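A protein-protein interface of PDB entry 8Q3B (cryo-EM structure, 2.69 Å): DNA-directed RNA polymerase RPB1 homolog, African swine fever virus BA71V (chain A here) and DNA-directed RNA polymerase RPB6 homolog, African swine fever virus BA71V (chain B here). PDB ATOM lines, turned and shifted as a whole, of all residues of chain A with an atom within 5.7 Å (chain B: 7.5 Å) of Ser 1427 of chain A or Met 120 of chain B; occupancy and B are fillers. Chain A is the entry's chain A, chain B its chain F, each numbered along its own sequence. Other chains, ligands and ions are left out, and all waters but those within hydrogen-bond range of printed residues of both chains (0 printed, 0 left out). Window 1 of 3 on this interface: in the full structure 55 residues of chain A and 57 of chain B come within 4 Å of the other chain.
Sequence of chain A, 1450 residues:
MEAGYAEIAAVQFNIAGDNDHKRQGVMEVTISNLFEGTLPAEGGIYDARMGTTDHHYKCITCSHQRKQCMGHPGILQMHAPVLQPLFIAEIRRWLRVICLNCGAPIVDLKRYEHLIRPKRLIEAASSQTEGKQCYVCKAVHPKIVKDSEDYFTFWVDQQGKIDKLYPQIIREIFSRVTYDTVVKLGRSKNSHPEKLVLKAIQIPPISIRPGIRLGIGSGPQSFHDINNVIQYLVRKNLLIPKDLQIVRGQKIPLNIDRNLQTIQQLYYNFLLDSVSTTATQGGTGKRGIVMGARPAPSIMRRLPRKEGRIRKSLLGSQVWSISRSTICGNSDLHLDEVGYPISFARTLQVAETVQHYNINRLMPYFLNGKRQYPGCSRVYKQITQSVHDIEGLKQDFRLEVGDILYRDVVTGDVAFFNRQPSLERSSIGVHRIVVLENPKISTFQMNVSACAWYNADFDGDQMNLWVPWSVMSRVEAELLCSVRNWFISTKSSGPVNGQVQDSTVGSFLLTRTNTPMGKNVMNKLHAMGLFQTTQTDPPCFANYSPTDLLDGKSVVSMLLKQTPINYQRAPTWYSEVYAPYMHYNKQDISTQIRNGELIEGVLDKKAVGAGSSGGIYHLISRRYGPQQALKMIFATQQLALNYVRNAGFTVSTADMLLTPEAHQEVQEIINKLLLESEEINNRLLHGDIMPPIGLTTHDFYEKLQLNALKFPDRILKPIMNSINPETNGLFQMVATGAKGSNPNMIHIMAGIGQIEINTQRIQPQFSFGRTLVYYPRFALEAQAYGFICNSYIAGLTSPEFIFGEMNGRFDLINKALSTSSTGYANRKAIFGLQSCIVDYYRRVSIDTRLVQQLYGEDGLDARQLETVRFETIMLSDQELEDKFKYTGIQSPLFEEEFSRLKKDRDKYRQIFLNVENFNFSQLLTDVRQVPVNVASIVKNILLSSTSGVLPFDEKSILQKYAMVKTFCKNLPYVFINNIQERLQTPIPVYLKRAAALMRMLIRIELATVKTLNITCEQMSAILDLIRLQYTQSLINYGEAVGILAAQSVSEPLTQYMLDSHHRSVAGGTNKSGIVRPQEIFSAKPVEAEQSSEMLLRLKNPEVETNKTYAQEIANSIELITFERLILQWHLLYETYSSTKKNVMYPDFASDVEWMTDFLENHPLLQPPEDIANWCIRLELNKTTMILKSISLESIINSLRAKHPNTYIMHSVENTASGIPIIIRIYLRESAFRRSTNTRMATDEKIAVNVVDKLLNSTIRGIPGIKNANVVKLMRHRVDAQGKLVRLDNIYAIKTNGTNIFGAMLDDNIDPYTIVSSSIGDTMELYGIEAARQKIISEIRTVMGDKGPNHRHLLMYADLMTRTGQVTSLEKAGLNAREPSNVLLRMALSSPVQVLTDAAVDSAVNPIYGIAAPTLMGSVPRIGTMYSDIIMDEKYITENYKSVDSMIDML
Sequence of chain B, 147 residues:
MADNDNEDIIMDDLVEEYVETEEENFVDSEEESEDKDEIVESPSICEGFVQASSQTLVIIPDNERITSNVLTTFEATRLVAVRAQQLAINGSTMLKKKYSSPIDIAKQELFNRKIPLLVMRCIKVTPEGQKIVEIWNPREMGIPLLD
OE2 of Glu 75 of chain B is in hydrogen-bond range of OG of Ser 1427 of chain A (2.8 Å). O of Asp 1428 of chain A is in hydrogen-bond range of N of Met 120 of chain B, at 2.9 Å. The backbone NH (N) of Leu 118 of chain B sits at hydrogen-bond distance from the backbone carbonyl oxygen (O) of Ile 1430 of chain A (2.6 Å).
The side-chain hydroxyl of Tyr 840 of chain A is in hydrogen-bond range of the side-chain hydroxyl of Ser 1427 of chain A (2.5 Å). OG1 of Thr 72 of chain B lies within hydrogen-bond range of N of Glu 75 of chain B, at 3.3 Å. The side-chain carboxylate (OE1) of Glu 75 of chain B lies within salt-bridge range of the guanidinium group (NH2) of Arg 121 of chain B (2.5 Å). O of Val 119 of chain B is in hydrogen-bond range of N of Trp 136 of chain B. The backbone NH (N) of Arg 121 of chain B sits at hydrogen-bond distance from the backbone carbonyl oxygen (O) of Glu 134 of chain B, at 2.8 Å. N of Ile 123 of chain B is in hydrogen-bond range of O of Ile 132 of chain B, 2.8 Å away.
Of the 19 printed residues of chain B, 11 touch a printed residue of chain A. Hydrophobic or aromatic side chains of chain B within 4 Å of the printed part of chain A: Phe 74, Leu 118, Met 120, Ile 123 and Ile 135. Among the printed residues, 18 pairs touch across the chains. Among the printed residues, no Asp or Glu carboxylate lies within 4 Å of a Lys or Arg side-chain nitrogen of the other chain.
Of chain B, only Glu 75, Met 120 and Arg 121 come within 4 Å of Ser 1427 of chain A. Of chain A, only Ser 1427 and Asp 1428 come within 4 Å of Met 120 of chain B. Of the printed residues of chain A, Cys 122 of chain B touches Tyr 840 (3.1 Å). Of the printed residues of chain A, Glu 75 of chain B touches Ser 1427 (2.8 Å). Printed residues of chain B within 4 Å of Tyr 1037 of chain A: Thr 72 (3.7 Å) and Arg 121 (3.99 Å). Of the printed residues of chain A, Val 119 of chain B touches Asp 1428. Of the printed residues of chain B, Met 1425 of chain A touches Arg 78 (3.8 Å). The nearest residue of chain A that does not touch Met 120 of chain B is Ile 1430 of chain A (4.1 Å).
Among the printed residues, merely in contact across the chains: Tyr 840 of chain A with Cys 122 of chain B (3.1 Å), Gly 1423 of chain A with Phe 74 of chain B (3.4 Å), Thr 1424 of chain A with Arg 78 of chain B (3.4 Å), Ile 1429 of chain A with Leu 118 of chain B (3.4 Å), Ile 1429 of chain A with Arg 78 of chain B (3.5 Å), Tyr 1037 of chain A with Thr 72 of chain B (3.7 Å), Tyr 840 of chain A with Arg 121 of chain B (3.7 Å), Asp 1428 of chain A with Val 119 of chain B (3.8 Å), Met 1425 of chain A with Arg 78 of chain B (3.8 Å), Ile 1430 of chain A with Ile 135 of chain B (3.8 Å), Thr 1424 of chain A with Phe 74 of chain B (3.8 Å), Ser 1427 of chain A with Met 120 of chain B (3.8 Å), Ser 1427 of chain A with Arg 121 of chain B (3.9 Å), Tyr 840 of chain A with Ile 123 of chain B (3.9 Å) and Tyr 1037 of chain A with Arg 121 of chain B (3.99 Å).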
ATOM      1  N   TYR A 840       6.045   6.935  21.832  1.00  0.00           N
ATOM      2  CA  TYR A 840       5.736   8.344  21.625  1.00  0.00           C
ATOM      3  C   TYR A 840       6.439   8.945  20.417  1.00  0.00           C
ATOM      4  O   TYR A 840       6.041  10.025  19.968  1.00  0.00           O
ATOM      5  CB  TYR A 840       6.093   9.135  22.881  1.00  0.00           C
ATOM      6  CG  TYR A 840       5.187   8.833  24.050  1.00  0.00           C
ATOM      7  CD1 TYR A 840       3.819   9.035  23.959  1.00  0.00           C
ATOM      8  CD2 TYR A 840       5.696   8.333  25.238  1.00  0.00           C
ATOM      9  CE1 TYR A 840       2.985   8.757  25.018  1.00  0.00           C
ATOM     10  CE2 TYR A 840       4.870   8.051  26.304  1.00  0.00           C
ATOM     11  CZ  TYR A 840       3.514   8.264  26.188  1.00  0.00           C
ATOM     12  OH  TYR A 840       2.684   7.986  27.248  1.00  0.00           O
ATOM     13  N   TYR A1037      -0.415   6.088  19.968  1.00  0.00           N
ATOM     14  CA  TYR A1037       0.825   6.011  20.727  1.00  0.00           C
ATOM     15  C   TYR A1037       0.902   4.803  21.650  1.00  0.00           C
ATOM     16  O   TYR A1037       1.915   4.637  22.335  1.00  0.00           O
ATOM     17  CB  TYR A1037       1.005   7.291  21.553  1.00  0.00           C
ATOM     18  CG  TYR A1037       1.598   8.463  20.796  1.00  0.00           C
ATOM     19  CD1 TYR A1037       2.495   8.270  19.753  1.00  0.00           C
ATOM     20  CD2 TYR A1037       1.249   9.765  21.121  1.00  0.00           C
ATOM     21  CE1 TYR A1037       3.030   9.335  19.069  1.00  0.00           C
ATOM     22  CE2 TYR A1037       1.780  10.836  20.437  1.00  0.00           C
ATOM     23  CZ  TYR A1037       2.669  10.614  19.412  1.00  0.00           C
ATOM     24  OH  TYR A1037       3.205  11.672  18.723  1.00  0.00           O
ATOM     25  N   GLY A1423      -2.225   1.000  25.035  1.00  0.00           N
ATOM     26  CA  GLY A1423      -3.583   1.425  24.738  1.00  0.00           C
ATOM     27  C   GLY A1423      -3.976   2.618  25.586  1.00  0.00           C
ATOM     28  O   GLY A1423      -3.271   3.632  25.633  1.00  0.00           O
ATOM     29  N   THR A1424      -5.117   2.506  26.267  1.00  0.00           N
ATOM     30  CA  THR A1424      -5.622   3.613  27.068  1.00  0.00           C
ATOM     31  C   THR A1424      -4.766   3.899  28.293  1.00  0.00           C
ATOM     32  O   THR A1424      -4.929   4.960  28.904  1.00  0.00           O
ATOM     33  CB  THR A1424      -7.057   3.330  27.514  1.00  0.00           C
ATOM     34  OG1 THR A1424      -7.157   1.981  27.982  1.00  0.00           O
ATOM     35  CG2 THR A1424      -8.026   3.537  26.365  1.00  0.00           C
ATOM     36  N   MET A1425      -3.864   2.991  28.665  1.00  0.00           N
ATOM     37  CA  MET A1425      -3.025   3.157  29.844  1.00  0.00           C
ATOM     38  C   MET A1425      -1.580   3.482  29.493  1.00  0.00           C
ATOM     39  O   MET A1425      -0.729   3.509  30.387  1.00  0.00           O
ATOM     40  CB  MET A1425      -3.074   1.899  30.714  1.00  0.00           C
ATOM     41  CG  MET A1425      -4.437   1.235  30.791  1.00  0.00           C
ATOM     42  SD  MET A1425      -5.518   2.080  31.953  1.00  0.00           S
ATOM     43  CE  MET A1425      -5.784   0.784  33.151  1.00  0.00           C
ATOM     44  N   TYR A1426      -1.278   3.725  28.217  1.00  0.00           N
ATOM     45  CA  TYR A1426       0.093   4.046  27.840  1.00  0.00           C
ATOM     46  C   TYR A1426       0.542   5.361  28.462  1.00  0.00           C
ATOM     47  O   TYR A1426       1.676   5.474  28.941  1.00  0.00           O
ATOM     48  CB  TYR A1426       0.219   4.108  26.319  1.00  0.00           C
ATOM     49  CG  TYR A1426       1.645   4.019  25.833  1.00  0.00           C
ATOM     50  CD1 TYR A1426       2.385   2.860  26.006  1.00  0.00           C
ATOM     51  CD2 TYR A1426       2.257   5.098  25.213  1.00  0.00           C
ATOM     52  CE1 TYR A1426       3.689   2.774  25.567  1.00  0.00           C
ATOM     53  CE2 TYR A1426       3.561   5.022  24.772  1.00  0.00           C
ATOM     54  CZ  TYR A1426       4.272   3.857  24.953  1.00  0.00           C
ATOM     55  OH  TYR A1426       5.572   3.775  24.517  1.00  0.00           O
ATOM     56  N   SER A1427      -0.332   6.362  28.470  1.00  0.00           N
ATOM     57  CA  SER A1427       0.003   7.695  28.948  1.00  0.00           C
ATOM     58  C   SER A1427      -0.618   7.936  30.318  1.00  0.00           C
ATOM     59  O   SER A1427      -1.794   7.638  30.540  1.00  0.00           O
ATOM     60  CB  SER A1427      -0.480   8.761  27.966  1.00  0.00           C
ATOM     61  OG  SER A1427       0.351   8.814  26.821  1.00  0.00           O
ATOM     62  N   ASP A1428       0.184   8.475  31.232  1.00  0.00           N
ATOM     63  CA  ASP A1428      -0.310   8.799  32.560  1.00  0.00           C
ATOM     64  C   ASP A1428      -1.223  10.018  32.509  1.00  0.00           C
ATOM     65  O   ASP A1428      -1.071  10.904  31.665  1.00  0.00           O
ATOM     66  CB  ASP A1428       0.853   9.070  33.512  1.00  0.00           C
ATOM     67  CG  ASP A1428       1.816   7.905  33.603  1.00  0.00           C
ATOM     68  OD1 ASP A1428       2.353   7.493  32.554  1.00  0.00           O
ATOM     69  OD2 ASP A1428       2.039   7.406  34.726  1.00  0.00           O
ATOM     70  N   ILE A1429      -2.182  10.054  33.429  1.00  0.00           N
ATOM     71  CA  ILE A1429      -3.073  11.192  33.609  1.00  0.00           C
ATOM     72  C   ILE A1429      -2.834  11.752  35.001  1.00  0.00           C
ATOM     73  O   ILE A1429      -2.901  11.015  35.991  1.00  0.00           O
ATOM     74  CB  ILE A1429      -4.552  10.800  33.427  1.00  0.00           C
ATOM     75  CG1 ILE A1429      -4.757  10.046  32.111  1.00  0.00           C
ATOM     76  CG2 ILE A1429      -5.439  12.033  33.471  1.00  0.00           C
ATOM     77  CD1 ILE A1429      -4.352  10.824  30.874  1.00  0.00           C
ATOM     78  N   ILE A1430      -2.550  13.048  35.075  1.00  0.00           N
ATOM     79  CA  ILE A1430      -2.335  13.732  36.342  1.00  0.00           C
ATOM     80  C   ILE A1430      -3.322  14.884  36.439  1.00  0.00           C
ATOM     81  O   ILE A1430      -3.758  15.444  35.429  1.00  0.00           O
ATOM     82  CB  ILE A1430      -0.881  14.232  36.489  1.00  0.00           C
ATOM     83  CG1 ILE A1430      -0.613  15.413  35.554  1.00  0.00           C
ATOM     84  CG2 ILE A1430       0.089  13.100  36.208  1.00  0.00           C
ATOM     85  CD1 ILE A1430       0.811  15.920  35.601  1.00  0.00           C
ATOM     86  N   LEU B  57      11.467  14.045  38.564  1.00  0.00           N
ATOM     87  CA  LEU B  57      10.639  14.298  37.392  1.00  0.00           C
ATOM     88  C   LEU B  57      11.215  15.463  36.598  1.00  0.00           C
ATOM     89  O   LEU B  57      11.258  16.595  37.091  1.00  0.00           O
ATOM     90  CB  LEU B  57       9.204  14.593  37.817  1.00  0.00           C
ATOM     91  CG  LEU B  57       8.131  14.411  36.745  1.00  0.00           C
ATOM     92  CD1 LEU B  57       7.804  12.940  36.559  1.00  0.00           C
ATOM     93  CD2 LEU B  57       6.886  15.198  37.109  1.00  0.00           C
ATOM     94  N   ILE B  59      10.581  17.711  33.531  1.00  0.00           N
ATOM     95  CA  ILE B  59       9.534  18.143  32.613  1.00  0.00           C
ATOM     96  C   ILE B  59      10.195  18.888  31.461  1.00  0.00           C
ATOM     97  O   ILE B  59      10.837  19.922  31.667  1.00  0.00           O
ATOM     98  CB  ILE B  59       8.501  19.027  33.327  1.00  0.00           C
ATOM     99  CG1 ILE B  59       7.845  18.247  34.468  1.00  0.00           C
ATOM    100  CG2 ILE B  59       7.448  19.519  32.341  1.00  0.00           C
ATOM    101  CD1 ILE B  59       6.895  19.068  35.316  1.00  0.00           C
ATOM    102  N   THR B  72      -4.398  11.447  21.047  1.00  0.00           N
ATOM    103  CA  THR B  72      -4.725  10.181  20.417  1.00  0.00           C
ATOM    104  C   THR B  72      -6.051   9.664  20.964  1.00  0.00           C
ATOM    105  O   THR B  72      -6.510  10.065  22.036  1.00  0.00           O
ATOM    106  CB  THR B  72      -3.619   9.152  20.654  1.00  0.00           C
ATOM    107  OG1 THR B  72      -3.526   8.853  22.051  1.00  0.00           O
ATOM    108  CG2 THR B  72      -2.282   9.679  20.159  1.00  0.00           C
ATOM    109  N   PHE B  74      -6.729   6.882  22.264  1.00  0.00           N
ATOM    110  CA  PHE B  74      -6.513   6.280  23.574  1.00  0.00           C
ATOM    111  C   PHE B  74      -6.485   7.341  24.665  1.00  0.00           C
ATOM    112  O   PHE B  74      -7.116   7.187  25.716  1.00  0.00           O
ATOM    113  CB  PHE B  74      -5.202   5.492  23.578  1.00  0.00           C
ATOM    114  CG  PHE B  74      -5.186   4.323  22.636  1.00  0.00           C
ATOM    115  CD1 PHE B  74      -6.308   3.536  22.455  1.00  0.00           C
ATOM    116  CD2 PHE B  74      -4.036   4.006  21.937  1.00  0.00           C
ATOM    117  CE1 PHE B  74      -6.282   2.461  21.593  1.00  0.00           C
ATOM    118  CE2 PHE B  74      -4.007   2.934  21.076  1.00  0.00           C
ATOM    119  CZ  PHE B  74      -5.130   2.161  20.903  1.00  0.00           C
ATOM    120  N   GLU B  75      -5.746   8.428  24.435  1.00  0.00           N
ATOM    121  CA  GLU B  75      -5.616   9.461  25.458  1.00  0.00           C
ATOM    122  C   GLU B  75      -6.942  10.167  25.706  1.00  0.00           C
ATOM    123  O   GLU B  75      -7.294  10.445  26.857  1.00  0.00           O
ATOM    124  CB  GLU B  75      -4.539  10.464  25.053  1.00  0.00           C
ATOM    125  CG  GLU B  75      -3.148  10.080  25.525  1.00  0.00           C
ATOM    126  CD  GLU B  75      -2.052  10.588  24.611  1.00  0.00           C
ATOM    127  OE1 GLU B  75      -2.335  11.457  23.762  1.00  0.00           O
ATOM    128  OE2 GLU B  75      -0.904  10.116  24.742  1.00  0.00           O
ATOM    129  N   ARG B  78      -9.128   7.794  27.702  1.00  0.00           N
ATOM    130  CA  ARG B  78      -8.683   7.709  29.089  1.00  0.00           C
ATOM    131  C   ARG B  78      -9.062   8.963  29.864  1.00  0.00           C
ATOM    132  O   ARG B  78      -9.514   8.880  31.012  1.00  0.00           O
ATOM    133  CB  ARG B  78      -7.172   7.477  29.135  1.00  0.00           C
ATOM    134  CG  ARG B  78      -6.566   7.497  30.529  1.00  0.00           C
ATOM    135  CD  ARG B  78      -6.931   6.254  31.316  1.00  0.00           C
ATOM    136  NE  ARG B  78      -6.230   6.199  32.592  1.00  0.00           N
ATOM    137  CZ  ARG B  78      -6.622   5.480  33.635  1.00  0.00           C
ATOM    138  NH1 ARG B  78      -7.708   4.727  33.588  1.00  0.00           N
ATOM    139  NH2 ARG B  78      -5.905   5.517  34.754  1.00  0.00           N
ATOM    140  N   LEU B 118      -4.578  16.581  33.194  1.00  0.00           N
ATOM    141  CA  LEU B 118      -3.415  16.783  32.346  1.00  0.00           C
ATOM    142  C   LEU B 118      -2.900  15.436  31.858  1.00  0.00           C
ATOM    143  O   LEU B 118      -3.113  14.399  32.490  1.00  0.00           O
ATOM    144  CB  LEU B 118      -2.295  17.521  33.091  1.00  0.00           C
ATOM    145  CG  LEU B 118      -2.562  18.961  33.527  1.00  0.00           C
ATOM    146  CD1 LEU B 118      -1.311  19.555  34.147  1.00  0.00           C
ATOM    147  CD2 LEU B 118      -3.032  19.812  32.362  1.00  0.00           C
ATOM    148  N   VAL B 119      -2.213  15.463  30.719  1.00  0.00           N
ATOM    149  CA  VAL B 119      -1.648  14.267  30.103  1.00  0.00           C
ATOM    150  C   VAL B 119      -0.139  14.317  30.290  1.00  0.00           C
ATOM    151  O   VAL B 119       0.510  15.296  29.905  1.00  0.00           O
ATOM    152  CB  VAL B 119      -2.014  14.166  28.614  1.00  0.00           C
ATOM    153  CG1 VAL B 119      -1.341  12.960  27.979  1.00  0.00           C
ATOM    154  CG2 VAL B 119      -3.518  14.085  28.444  1.00  0.00           C
ATOM    155  N   MET B 120       0.415  13.263  30.880  1.00  0.00           N
ATOM    156  CA  MET B 120       1.852  13.128  31.077  1.00  0.00           C
ATOM    157  C   MET B 120       2.352  11.998  30.188  1.00  0.00           C
ATOM    158  O   MET B 120       1.875  10.864  30.295  1.00  0.00           O
ATOM    159  CB  MET B 120       2.179  12.851  32.544  1.00  0.00           C
ATOM    160  CG  MET B 120       3.658  12.655  32.836  1.00  0.00           C
ATOM    161  SD  MET B 120       3.944  11.894  34.442  1.00  0.00           S
ATOM    162  CE  MET B 120       4.106  13.347  35.472  1.00  0.00           C
ATOM    163  N   ARG B 121       3.306  12.308  29.319  1.00  0.00           N
ATOM    164  CA  ARG B 121       3.860  11.351  28.365  1.00  0.00           C
ATOM    165  C   ARG B 121       5.301  11.068  28.772  1.00  0.00           C
ATOM    166  O   ARG B 121       6.194  11.885  28.536  1.00  0.00           O
ATOM    167  CB  ARG B 121       3.769  11.898  26.944  1.00  0.00           C
ATOM    168  CG  ARG B 121       2.344  12.108  26.464  1.00  0.00           C
ATOM    169  CD  ARG B 121       2.297  12.702  25.068  1.00  0.00           C
ATOM    170  NE  ARG B 121       0.956  12.646  24.500  1.00  0.00           N
ATOM    171  CZ  ARG B 121       0.577  13.296  23.407  1.00  0.00           C
ATOM    172  NH1 ARG B 121       1.411  14.076  22.742  1.00  0.00           N
ATOM    173  NH2 ARG B 121      -0.671  13.158  22.972  1.00  0.00           N
ATOM    174  N   CYS B 122       5.523   9.906  29.380  1.00  0.00           N
ATOM    175  CA  CYS B 122       6.852   9.537  29.857  1.00  0.00           C
ATOM    176  C   CYS B 122       7.740   9.200  28.669  1.00  0.00           C
ATOM    177  O   CYS B 122       7.525   8.195  27.984  1.00  0.00           O
ATOM    178  CB  CYS B 122       6.757   8.358  30.820  1.00  0.00           C
ATOM    179  SG  CYS B 122       8.346   7.842  31.509  1.00  0.00           S
ATOM    180  N   ILE B 123       8.746  10.035  28.425  1.00  0.00           N
ATOM    181  CA  ILE B 123       9.634   9.849  27.284  1.00  0.00           C
ATOM    182  C   ILE B 123      10.777   8.903  27.620  1.00  0.00           C
ATOM    183  O   ILE B 123      11.079   7.984  26.854  1.00  0.00           O
ATOM    184  CB  ILE B 123      10.166  11.216  26.803  1.00  0.00           C
ATOM    185  CG1 ILE B 123       9.018  12.110  26.324  1.00  0.00           C
ATOM    186  CG2 ILE B 123      11.186  11.028  25.691  1.00  0.00           C
ATOM    187  CD1 ILE B 123       8.151  11.498  25.242  1.00  0.00           C
ATOM    188  N   LYS B 131      13.199  10.815  35.414  1.00  0.00           N
ATOM    189  CA  LYS B 131      12.044  10.445  34.604  1.00  0.00           C
ATOM    190  C   LYS B 131      11.726  11.645  33.722  1.00  0.00           C
ATOM    191  O   LYS B 131      11.115  12.615  34.177  1.00  0.00           O
ATOM    192  CB  LYS B 131      10.858  10.057  35.482  1.00  0.00           C
ATOM    193  CG  LYS B 131       9.805   9.227  34.770  1.00  0.00           C
ATOM    194  CD  LYS B 131       8.596   8.993  35.655  1.00  0.00           C
ATOM    195  CE  LYS B 131       7.601   8.052  35.002  1.00  0.00           C
ATOM    196  NZ  LYS B 131       6.374   7.879  35.825  1.00  0.00           N
ATOM    197  N   ILE B 132      12.171  11.590  32.471  1.00  0.00           N
ATOM    198  CA  ILE B 132      11.976  12.678  31.521  1.00  0.00           C
ATOM    199  C   ILE B 132      10.617  12.490  30.865  1.00  0.00           C
ATOM    200  O   ILE B 132      10.390  11.494  30.164  1.00  0.00           O
ATOM    201  CB  ILE B 132      13.097  12.709  30.473  1.00  0.00           C
ATOM    202  CG1 ILE B 132      14.464  12.650  31.162  1.00  0.00           C
ATOM    203  CG2 ILE B 132      12.980  13.956  29.608  1.00  0.00           C
ATOM    204  CD1 ILE B 132      15.638  12.682  30.212  1.00  0.00           C
ATOM    205  N   VAL B 133       9.719  13.454  31.085  1.00  0.00           N
ATOM    206  CA  VAL B 133       8.331  13.366  30.652  1.00  0.00           C
ATOM    207  C   VAL B 133       7.931  14.674  29.982  1.00  0.00           C
ATOM    208  O   VAL B 133       8.594  15.704  30.125  1.00  0.00           O
ATOM    209  CB  VAL B 133       7.378  13.062  31.828  1.00  0.00           C
ATOM    210  CG1 VAL B 133       7.921  11.925  32.675  1.00  0.00           C
ATOM    211  CG2 VAL B 133       7.166  14.305  32.679  1.00  0.00           C
ATOM    212  N   GLU B 134       6.825  14.618  29.243  1.00  0.00           N
ATOM    213  CA  GLU B 134       6.213  15.789  28.630  1.00  0.00           C
ATOM    214  C   GLU B 134       4.808  15.962  29.185  1.00  0.00           C
ATOM    215  O   GLU B 134       4.007  15.023  29.153  1.00  0.00           O
ATOM    216  CB  GLU B 134       6.158  15.658  27.107  1.00  0.00           C
ATOM    217  CG  GLU B 134       7.508  15.472  26.448  1.00  0.00           C
ATOM    218  CD  GLU B 134       7.405  15.325  24.945  1.00  0.00           C
ATOM    219  OE1 GLU B 134       6.295  15.503  24.405  1.00  0.00           O
ATOM    220  OE2 GLU B 134       8.435  15.032  24.304  1.00  0.00           O
ATOM    221  N   ILE B 135       4.513  17.157  29.685  1.00  0.00           N
ATOM    222  CA  ILE B 135       3.202  17.479  30.237  1.00  0.00           C
ATOM    223  C   ILE B 135       2.416  18.230  29.174  1.00  0.00           C
ATOM    224  O   ILE B 135       2.847  19.287  28.700  1.00  0.00           O
ATOM    225  CB  ILE B 135       3.320  18.310  31.524  1.00  0.00           C
ATOM    226  CG1 ILE B 135       4.228  17.610  32.540  1.00  0.00           C
ATOM    227  CG2 ILE B 135       1.943  18.560  32.119  1.00  0.00           C
ATOM    228  CD1 ILE B 135       3.662  16.322  33.095  1.00  0.00           C
ATOM    229  N   TRP B 136       1.262  17.685  28.800  1.00  0.00           N
ATOM    230  CA  TRP B 136       0.408  18.264  27.774  1.00  0.00           C
ATOM    231  C   TRP B 136      -0.933  18.649  28.379  1.00  0.00           C
ATOM    232  O   TRP B 136      -1.509  17.895  29.169  1.00  0.00           O
ATOM    233  CB  TRP B 136       0.195  17.286  26.619  1.00  0.00           C
ATOM    234  CG  TRP B 136       1.329  17.251  25.650  1.00  0.00           C
ATOM    235  CD1 TRP B 136       2.402  16.410  25.671  1.00  0.00           C
ATOM    236  CD2 TRP B 136       1.510  18.103  24.514  1.00  0.00           C
ATOM    237  NE1 TRP B 136       3.237  16.683  24.616  1.00  0.00           N
ATOM    238  CE2 TRP B 136       2.712  17.719  23.892  1.00  0.00           C
ATOM    239  CE3 TRP B 136       0.771  19.154  23.965  1.00  0.00           C
ATOM    240  CZ2 TRP B 136       3.191  18.348  22.748  1.00  0.00           C
ATOM    241  CZ3 TRP B 136       1.248  19.775  22.829  1.00  0.00           C
ATOM    242  CH2 TRP B 136       2.445  19.372  22.234  1.00  0.00           C
ATOM    243  N   ASN B 137      -1.429  19.825  27.999  1.00  0.00           N
ATOM    244  CA  ASN B 137      -2.696  20.321  28.514  1.00  0.00           C
ATOM    245  C   ASN B 137      -3.815  19.949  27.550  1.00  0.00           C
ATOM    246  O   ASN B 137      -3.811  20.421  26.406  1.00  0.00           O
ATOM    247  CB  ASN B 137      -2.644  21.827  28.693  1.00  0.00           C
ATOM    248  CG  ASN B 137      -3.856  22.368  29.419  1.00  0.00           C
ATOM    249  OD1 ASN B 137      -4.732  21.612  29.833  1.00  0.00           O
ATOM    250  ND2 ASN B 137      -3.909  23.684  29.579  1.00  0.00           N
